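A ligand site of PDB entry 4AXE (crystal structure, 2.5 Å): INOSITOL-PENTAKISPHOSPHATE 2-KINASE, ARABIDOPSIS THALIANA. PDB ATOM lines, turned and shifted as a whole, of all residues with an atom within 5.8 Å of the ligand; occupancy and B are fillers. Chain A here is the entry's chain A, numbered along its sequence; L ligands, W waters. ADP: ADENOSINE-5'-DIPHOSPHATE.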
ATOM      1  N   ARG A  21      20.215 -31.106 -24.404  1.00  0.00           N
ATOM      2  CA  ARG A  21      21.509 -30.765 -23.863  1.00  0.00           C
ATOM      3  C   ARG A  21      21.545 -30.995 -22.353  1.00  0.00           C
ATOM      4  O   ARG A  21      22.453 -31.643 -21.835  1.00  0.00           O
ATOM      5  CB  ARG A  21      21.865 -29.317 -24.202  1.00  0.00           C
ATOM      6  CG  ARG A  21      23.080 -28.767 -23.471  1.00  0.00           C
ATOM      7  CD  ARG A  21      24.371 -29.470 -23.861  1.00  0.00           C
ATOM      8  NE  ARG A  21      24.673 -29.323 -25.285  1.00  0.00           N
ATOM      9  CZ  ARG A  21      25.217 -28.250 -25.848  1.00  0.00           C
ATOM     10  NH1 ARG A  21      25.533 -27.185 -25.111  1.00  0.00           N
ATOM     11  NH2 ARG A  21      25.450 -28.233 -27.149  1.00  0.00           N
ATOM     12  N   GLY A  22      20.538 -30.465 -21.663  1.00  0.00           N
ATOM     13  CA  GLY A  22      20.462 -30.612 -20.210  1.00  0.00           C
ATOM     14  C   GLY A  22      19.190 -30.092 -19.589  1.00  0.00           C
ATOM     15  O   GLY A  22      18.251 -29.715 -20.272  1.00  0.00           O
ATOM     16  N   GLU A  23      19.173 -30.080 -18.257  1.00  0.00           N
ATOM     17  CA  GLU A  23      18.028 -29.625 -17.494  1.00  0.00           C
ATOM     18  C   GLU A  23      18.405 -29.350 -16.046  1.00  0.00           C
ATOM     19  O   GLU A  23      19.380 -29.910 -15.527  1.00  0.00           O
ATOM     20  CB  GLU A  23      16.866 -30.630 -17.563  1.00  0.00           C
ATOM     21  CG  GLU A  23      17.132 -31.992 -16.927  1.00  0.00           C
ATOM     22  CD  GLU A  23      15.997 -32.971 -17.152  1.00  0.00           C
ATOM     23  OE1 GLU A  23      15.996 -33.652 -18.208  1.00  0.00           O
ATOM     24  OE2 GLU A  23      15.103 -33.065 -16.286  1.00  0.00           O
ATOM     25  N   GLY A  24      17.642 -28.467 -15.413  1.00  0.00           N
ATOM     26  CA  GLY A  24      17.735 -28.272 -13.973  1.00  0.00           C
ATOM     27  C   GLY A  24      16.382 -28.555 -13.351  1.00  0.00           C
ATOM     28  O   GLY A  24      15.605 -29.378 -13.859  1.00  0.00           O
ATOM     29  N   GLY A  25      16.090 -27.875 -12.246  1.00  0.00           N
ATOM     30  CA  GLY A  25      14.805 -28.033 -11.567  1.00  0.00           C
ATOM     31  C   GLY A  25      13.633 -27.341 -12.260  1.00  0.00           C
ATOM     32  O   GLY A  25      12.487 -27.756 -12.094  1.00  0.00           O
ATOM     33  N   ALA A  26      13.917 -26.298 -13.034  1.00  0.00           N
ATOM     34  CA  ALA A  26      12.861 -25.488 -13.645  1.00  0.00           C
ATOM     35  C   ALA A  26      12.826 -25.509 -15.178  1.00  0.00           C
ATOM     36  O   ALA A  26      11.771 -25.268 -15.781  1.00  0.00           O
ATOM     37  CB  ALA A  26      12.948 -24.047 -13.148  1.00  0.00           C
ATOM     38  N   ASN A  27      13.963 -25.812 -15.805  1.00  0.00           N
ATOM     39  CA  ASN A  27      14.106 -25.660 -17.262  1.00  0.00           C
ATOM     40  C   ASN A  27      14.757 -26.831 -18.004  1.00  0.00           C
ATOM     41  O   ASN A  27      15.673 -27.472 -17.496  1.00  0.00           O
ATOM     42  CB  ASN A  27      14.895 -24.392 -17.566  1.00  0.00           C
ATOM     43  CG  ASN A  27      14.198 -23.139 -17.083  1.00  0.00           C
ATOM     44  OD1 ASN A  27      13.219 -22.698 -17.686  1.00  0.00           O
ATOM     45  ND2 ASN A  27      14.697 -22.572 -15.988  1.00  0.00           N
ATOM     46  N   LEU A  28      14.242 -27.094 -19.207  1.00  0.00           N
ATOM     47  CA  LEU A  28      14.897 -27.965 -20.177  1.00  0.00           C
ATOM     48  C   LEU A  28      15.766 -27.110 -21.094  1.00  0.00           C
ATOM     49  O   LEU A  28      15.408 -25.966 -21.427  1.00  0.00           O
ATOM     50  CB  LEU A  28      13.872 -28.724 -21.027  1.00  0.00           C
ATOM     51  CG  LEU A  28      13.178 -30.037 -20.594  1.00  0.00           C
ATOM     52  CD1 LEU A  28      14.029 -30.898 -19.669  1.00  0.00           C
ATOM     53  CD2 LEU A  28      11.811 -29.777 -19.988  1.00  0.00           C
ATOM     54  N   VAL A  29      16.911 -27.650 -21.514  1.00  0.00           N
ATOM     55  CA  VAL A  29      17.785 -26.952 -22.441  1.00  0.00           C
ATOM     56  C   VAL A  29      18.115 -27.813 -23.647  1.00  0.00           C
ATOM     57  O   VAL A  29      18.661 -28.916 -23.504  1.00  0.00           O
ATOM     58  CB  VAL A  29      19.079 -26.465 -21.760  1.00  0.00           C
ATOM     59  CG1 VAL A  29      19.985 -25.754 -22.776  1.00  0.00           C
ATOM     60  CG2 VAL A  29      18.765 -25.544 -20.594  1.00  0.00           C
ATOM     61  N   VAL A  43      21.186 -22.036 -27.872  1.00  0.00           N
ATOM     62  CA  VAL A  43      20.359 -23.019 -27.171  1.00  0.00           C
ATOM     63  C   VAL A  43      18.969 -22.435 -26.941  1.00  0.00           C
ATOM     64  O   VAL A  43      18.783 -21.215 -26.990  1.00  0.00           O
ATOM     65  CB  VAL A  43      20.964 -23.474 -25.823  1.00  0.00           C
ATOM     66  CG1 VAL A  43      22.230 -24.311 -26.046  1.00  0.00           C
ATOM     67  CG2 VAL A  43      21.232 -22.291 -24.900  1.00  0.00           C
ATOM     68  N   ARG A  45      15.825 -22.451 -24.078  1.00  0.00           N
ATOM     69  CA  ARG A  45      15.490 -22.732 -22.689  1.00  0.00           C
ATOM     70  C   ARG A  45      13.982 -22.751 -22.551  1.00  0.00           C
ATOM     71  O   ARG A  45      13.312 -21.738 -22.804  1.00  0.00           O
ATOM     72  CB  ARG A  45      16.109 -21.689 -21.772  1.00  0.00           C
ATOM     73  CG  ARG A  45      16.444 -22.184 -20.372  1.00  0.00           C
ATOM     74  CD  ARG A  45      16.588 -21.003 -19.419  1.00  0.00           C
ATOM     75  NE  ARG A  45      17.155 -21.376 -18.130  1.00  0.00           N
ATOM     76  CZ  ARG A  45      17.085 -20.624 -17.033  1.00  0.00           C
ATOM     77  NH1 ARG A  45      16.452 -19.451 -17.065  1.00  0.00           N
ATOM     78  NH2 ARG A  45      17.633 -21.025 -15.900  1.00  0.00           N
ATOM     79  N   LYS A  48       9.753 -26.070 -17.468  1.00  0.00           N
ATOM     80  CA  LYS A  48       9.011 -27.258 -17.062  1.00  0.00           C
ATOM     81  C   LYS A  48       7.680 -26.890 -16.437  1.00  0.00           C
ATOM     82  O   LYS A  48       7.553 -25.819 -15.829  1.00  0.00           O
ATOM     83  CB  LYS A  48       9.832 -28.073 -16.049  1.00  0.00           C
ATOM     84  CG  LYS A  48      11.130 -28.654 -16.578  1.00  0.00           C
ATOM     85  CD  LYS A  48      11.910 -29.334 -15.465  1.00  0.00           C
ATOM     86  CE  LYS A  48      13.070 -30.136 -16.029  1.00  0.00           C
ATOM     87  NZ  LYS A  48      13.779 -30.903 -14.971  1.00  0.00           N
ATOM     88  N   LEU A 151      19.285 -18.452 -26.202  1.00  0.00           N
ATOM     89  CA  LEU A 151      20.536 -18.010 -25.577  1.00  0.00           C
ATOM     90  C   LEU A 151      21.739 -18.480 -26.385  1.00  0.00           C
ATOM     91  O   LEU A 151      21.672 -19.500 -27.054  1.00  0.00           O
ATOM     92  CB  LEU A 151      20.652 -18.591 -24.166  1.00  0.00           C
ATOM     93  CG  LEU A 151      19.693 -18.127 -23.070  1.00  0.00           C
ATOM     94  CD1 LEU A 151      19.484 -19.258 -22.059  1.00  0.00           C
ATOM     95  CD2 LEU A 151      20.218 -16.876 -22.377  1.00  0.00           C
ATOM     96  N   ASN A 152      22.846 -17.725 -26.323  1.00  0.00           N
ATOM     97  CA  ASN A 152      24.109 -18.213 -26.869  1.00  0.00           C
ATOM     98  C   ASN A 152      24.545 -19.466 -26.114  1.00  0.00           C
ATOM     99  O   ASN A 152      24.506 -19.514 -24.882  1.00  0.00           O
ATOM    100  CB  ASN A 152      25.205 -17.142 -26.778  1.00  0.00           C
ATOM    101  CG  ASN A 152      25.016 -16.029 -27.787  1.00  0.00           C
ATOM    102  OD1 ASN A 152      24.828 -14.867 -27.414  1.00  0.00           O
ATOM    103  ND2 ASN A 152      25.066 -16.359 -29.078  1.00  0.00           N
ATOM    104  N   ASP A 153      24.940 -20.498 -26.869  1.00  0.00           N
ATOM    105  CA  ASP A 153      25.478 -21.727 -26.302  1.00  0.00           C
ATOM    106  C   ASP A 153      26.866 -21.422 -25.739  1.00  0.00           C
ATOM    107  O   ASP A 153      27.829 -21.250 -26.496  1.00  0.00           O
ATOM    108  CB  ASP A 153      25.526 -22.820 -27.380  1.00  0.00           C
ATOM    109  CG  ASP A 153      26.020 -24.164 -26.855  1.00  0.00           C
ATOM    110  OD1 ASP A 153      26.362 -24.301 -25.661  1.00  0.00           O
ATOM    111  OD2 ASP A 153      26.072 -25.121 -27.663  1.00  0.00           O
ATOM    112  N   HIS A 154      26.957 -21.324 -24.417  1.00  0.00           N
ATOM    113  CA  HIS A 154      28.211 -20.989 -23.748  1.00  0.00           C
ATOM    114  C   HIS A 154      29.175 -22.147 -23.651  1.00  0.00           C
ATOM    115  O   HIS A 154      30.279 -22.017 -23.118  1.00  0.00           O
ATOM    116  CB  HIS A 154      27.959 -20.375 -22.377  1.00  0.00           C
ATOM    117  CG  HIS A 154      27.100 -19.129 -22.411  1.00  0.00           C
ATOM    118  ND1 HIS A 154      27.270 -18.160 -23.327  1.00  0.00           N
ATOM    119  CD2 HIS A 154      26.060 -18.703 -21.582  1.00  0.00           C
ATOM    120  CE1 HIS A 154      26.376 -17.168 -23.109  1.00  0.00           C
ATOM    121  NE2 HIS A 154      25.647 -17.504 -22.036  1.00  0.00           N
ATOM    122  N   SER A 155      28.763 -23.310 -24.173  1.00  0.00           N
ATOM    123  CA  SER A 155      29.676 -24.431 -24.329  1.00  0.00           C
ATOM    124  C   SER A 155      30.465 -24.282 -25.634  1.00  0.00           C
ATOM    125  O   SER A 155      31.343 -25.087 -25.925  1.00  0.00           O
ATOM    126  CB  SER A 155      28.926 -25.766 -24.296  1.00  0.00           C
ATOM    127  OG  SER A 155      28.340 -26.057 -25.554  1.00  0.00           O
ATOM    128  N   GLU A 171      31.754 -26.063 -16.685  1.00  0.00           N
ATOM    129  CA  GLU A 171      30.620 -25.544 -15.942  1.00  0.00           C
ATOM    130  C   GLU A 171      30.752 -25.812 -14.452  1.00  0.00           C
ATOM    131  O   GLU A 171      30.855 -26.969 -14.026  1.00  0.00           O
ATOM    132  CB  GLU A 171      29.319 -26.130 -16.479  1.00  0.00           C
ATOM    133  CG  GLU A 171      28.074 -25.532 -15.834  1.00  0.00           C
ATOM    134  CD  GLU A 171      26.795 -26.212 -16.293  1.00  0.00           C
ATOM    135  OE1 GLU A 171      26.808 -26.843 -17.366  1.00  0.00           O
ATOM    136  OE2 GLU A 171      25.790 -26.121 -15.579  1.00  0.00           O
ATOM    137  N   ARG A 246      31.210 -29.899 -14.415  1.00  0.00           N
ATOM    138  CA  ARG A 246      30.973 -30.567 -15.705  1.00  0.00           C
ATOM    139  C   ARG A 246      31.969 -30.044 -16.713  1.00  0.00           C
ATOM    140  O   ARG A 246      32.383 -28.883 -16.643  1.00  0.00           O
ATOM    141  CB  ARG A 246      29.577 -30.238 -16.249  1.00  0.00           C
ATOM    142  CG  ARG A 246      28.392 -30.729 -15.435  1.00  0.00           C
ATOM    143  CD  ARG A 246      27.218 -29.798 -15.680  1.00  0.00           C
ATOM    144  NE  ARG A 246      25.925 -30.451 -15.485  1.00  0.00           N
ATOM    145  CZ  ARG A 246      25.248 -30.462 -14.346  1.00  0.00           C
ATOM    146  NH1 ARG A 246      25.717 -29.853 -13.267  1.00  0.00           N
ATOM    147  NH2 ARG A 246      24.081 -31.081 -14.293  1.00  0.00           N
ATOM    148  N   PHE A 248      32.539 -29.925 -21.063  1.00  0.00           N
ATOM    149  CA  PHE A 248      31.977 -30.161 -22.389  1.00  0.00           C
ATOM    150  C   PHE A 248      33.048 -30.091 -23.487  1.00  0.00           C
ATOM    151  O   PHE A 248      33.963 -29.261 -23.417  1.00  0.00           O
ATOM    152  CB  PHE A 248      30.865 -29.152 -22.696  1.00  0.00           C
ATOM    153  CG  PHE A 248      29.696 -29.223 -21.761  1.00  0.00           C
ATOM    154  CD1 PHE A 248      28.653 -30.107 -22.002  1.00  0.00           C
ATOM    155  CD2 PHE A 248      29.627 -28.400 -20.647  1.00  0.00           C
ATOM    156  CE1 PHE A 248      27.552 -30.176 -21.143  1.00  0.00           C
ATOM    157  CE2 PHE A 248      28.540 -28.466 -19.786  1.00  0.00           C
ATOM    158  CZ  PHE A 248      27.507 -29.357 -20.032  1.00  0.00           C
ATOM    159  N   MET A 377      29.971 -20.678 -16.627  1.00  0.00           N
ATOM    160  CA  MET A 377      30.471 -21.467 -17.738  1.00  0.00           C
ATOM    161  C   MET A 377      31.681 -20.760 -18.335  1.00  0.00           C
ATOM    162  O   MET A 377      31.591 -19.613 -18.808  1.00  0.00           O
ATOM    163  CB  MET A 377      29.381 -21.691 -18.807  1.00  0.00           C
ATOM    164  CG  MET A 377      28.253 -22.621 -18.365  1.00  0.00           C
ATOM    165  SD  MET A 377      27.168 -23.118 -19.726  1.00  0.00           S
ATOM    166  CE  MET A 377      28.089 -24.495 -20.409  1.00  0.00           C
ATOM    167  N   ILE A 411      25.112 -18.506 -15.794  1.00  0.00           N
ATOM    168  CA  ILE A 411      23.811 -19.087 -16.163  1.00  0.00           C
ATOM    169  C   ILE A 411      22.972 -19.395 -14.924  1.00  0.00           C
ATOM    170  O   ILE A 411      23.493 -19.376 -13.809  1.00  0.00           O
ATOM    171  CB  ILE A 411      23.944 -20.359 -17.045  1.00  0.00           C
ATOM    172  CG1 ILE A 411      24.552 -21.507 -16.244  1.00  0.00           C
ATOM    173  CG2 ILE A 411      24.708 -20.040 -18.327  1.00  0.00           C
ATOM    174  CD1 ILE A 411      24.404 -22.867 -16.899  1.00  0.00           C
ATOM    175  N   ASP A 412      21.690 -19.676 -15.148  1.00  0.00           N
ATOM    176  CA  ASP A 412      20.765 -20.124 -14.105  1.00  0.00           C
ATOM    177  C   ASP A 412      20.589 -19.068 -13.012  1.00  0.00           C
ATOM    178  O   ASP A 412      20.615 -19.372 -11.817  1.00  0.00           O
ATOM    179  CB  ASP A 412      21.223 -21.467 -13.516  1.00  0.00           C
ATOM    180  CG  ASP A 412      20.104 -22.242 -12.850  1.00  0.00           C
ATOM    181  OD1 ASP A 412      18.917 -22.078 -13.241  1.00  0.00           O
ATOM    182  OD2 ASP A 412      20.394 -23.030 -11.931  1.00  0.00           O
ATOM    183  N   SER A 414      18.059 -17.299 -11.688  1.00  0.00           N
ATOM    184  CA  SER A 414      16.599 -17.231 -11.565  1.00  0.00           C
ATOM    185  C   SER A 414      16.108 -16.434 -10.368  1.00  0.00           C
ATOM    186  O   SER A 414      16.769 -16.376  -9.328  1.00  0.00           O
ATOM    187  CB  SER A 414      15.995 -18.648 -11.529  1.00  0.00           C
ATOM    188  OG  SER A 414      16.600 -19.432 -10.517  1.00  0.00           O
HETATM  189  PB  ADP L   1      17.398 -24.787 -14.522  1.00  0.00           P
HETATM  190  O1B ADP L   1      18.373 -25.020 -13.383  1.00  0.00           O
HETATM  191  O2B ADP L   1      17.002 -23.342 -14.724  1.00  0.00           O
HETATM  192  O3B ADP L   1      16.216 -25.741 -14.522  1.00  0.00           O
HETATM  193  PA  ADP L   1      19.542 -24.378 -16.360  1.00  0.00           P
HETATM  194  O1A ADP L   1      19.064 -23.132 -17.050  1.00  0.00           O
HETATM  195  O2A ADP L   1      20.573 -24.305 -15.256  1.00  0.00           O
HETATM  196  O3A ADP L   1      18.234 -25.190 -15.842  1.00  0.00           O
HETATM  197  O5' ADP L   1      20.124 -25.362 -17.484  1.00  0.00           O
HETATM  198  C5' ADP L   1      20.425 -26.720 -17.188  1.00  0.00           C
HETATM  199  C4' ADP L   1      21.674 -27.158 -17.937  1.00  0.00           C
HETATM  200  O4' ADP L   1      21.617 -26.745 -19.320  1.00  0.00           O
HETATM  201  C3' ADP L   1      22.923 -26.525 -17.350  1.00  0.00           C
HETATM  202  O3' ADP L   1      23.490 -27.356 -16.317  1.00  0.00           O
HETATM  203  C2' ADP L   1      23.826 -26.328 -18.549  1.00  0.00           C
HETATM  204  O2' ADP L   1      24.640 -27.493 -18.744  1.00  0.00           O
HETATM  205  C1' ADP L   1      22.891 -26.216 -19.727  1.00  0.00           C
HETATM  206  N9  ADP L   1      22.778 -24.791 -20.145  1.00  0.00           N
HETATM  207  C8  ADP L   1      21.944 -23.878 -19.632  1.00  0.00           C
HETATM  208  N7  ADP L   1      22.105 -22.669 -20.240  1.00  0.00           N
HETATM  209  C5  ADP L   1      23.065 -22.809 -21.168  1.00  0.00           C
HETATM  210  C6  ADP L   1      23.725 -21.929 -22.178  1.00  0.00           C
HETATM  211  N6  ADP L   1      23.391 -20.629 -22.324  1.00  0.00           N
HETATM  212  N1  ADP L   1      24.674 -22.485 -22.952  1.00  0.00           N
HETATM  213  C2  ADP L   1      25.029 -23.787 -22.831  1.00  0.00           C
HETATM  214  N3  ADP L   1      24.477 -24.632 -21.947  1.00  0.00           N
HETATM  215  C4  ADP L   1      23.502 -24.212 -21.100  1.00  0.00           C
HETATM  216  O   HOH W   1      22.066 -28.865 -14.490  1.00  0.00           O
HETATM  217  O   HOH W   2      19.054 -26.805 -11.214  1.00  0.00           O
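An oxygen (O3B) of the ligand is in hydrogen-bond range of the backbone NH of Asn 27. ND2 of Asn 27 sits at hydrogen-bond distance from O2B of the ligand (2.7 Å). The side-chain carboxylate of Glu 171 is in hydrogen-bond range of an oxygen (O2') of the ligand (2.6 Å). The guanidinium group (NH2) of Arg 45 is in salt-bridge range of an oxygen (O2B) of the ligand (2.7 Å). The side-chain carboxylate (OD1) of Asp 412 sits close to an oxygen (O2B) of the ligand, 2.7 Å away. N of Ala 26 sits at hydrogen-bond distance from O3B of the ligand, at 2.8 Å. N1 of the ligand is in hydrogen-bond range of N of His 154 (3.0 Å). The backbone NH of Gly 24 lies close to an oxygen (O3B) of the ligand (3.2 Å). O of Asn 152 sits at hydrogen-bond distance from N6 of the ligand (3.0 Å). The backbone NH (N) of Gly 25 lies within hydrogen-bond range of an oxygen (O3B) of the ligand, 3.1 Å away.
Water W1 lies within hydrogen-bond range of an oxygen (O3') of the ligand (2.8 Å), the guanidinium group of Arg 246 (3.0 Å) and the backbone carbonyl oxygen of Glu 23 (3.1 Å). Water W2 lies within hydrogen-bond range of O1B of the ligand (2.9 Å) and N of Gly 25 (3.3 Å).
The side-chain amide nitrogen (ND2) of Asn 27 lies close to the guanidinium group (NH2) of Arg 45 (3.3 Å). O of Arg 246 lies within hydrogen-bond range of N of Glu 171 (2.9 Å). The side-chain carboxylate (OD1) of Asp 412 is in salt-bridge range of the guanidinium group (NH2) of Arg 45, 3.1 Å away. The backbone carbonyl oxygen (O) of Ala 26 lies within hydrogen-bond range of the backbone NH (N) of Lys 48, at 2.7 Å. The backbone carbonyl oxygen of Gly 24 is in hydrogen-bond range of the side-chain amino group of Lys 48, at 2.6 Å. The side-chain hydroxyl (OG) of Ser 155 sits at hydrogen-bond distance from the side-chain carboxylate (OD1) of Asp 153. The backbone carbonyl oxygen (O) of Leu 151 is in hydrogen-bond range of the backbone NH (N) of Val 43 (2.7 Å). The guanidinium group of Arg 21 lies within hydrogen-bond range of the side-chain hydroxyl of Ser 155, 3.1 Å away.
Merely in contact with the ligand: Asp 153, Val 29, Glu 23, Phe 248, Val 43, Met 377, Ile 411, Leu 151 and Ser 155.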
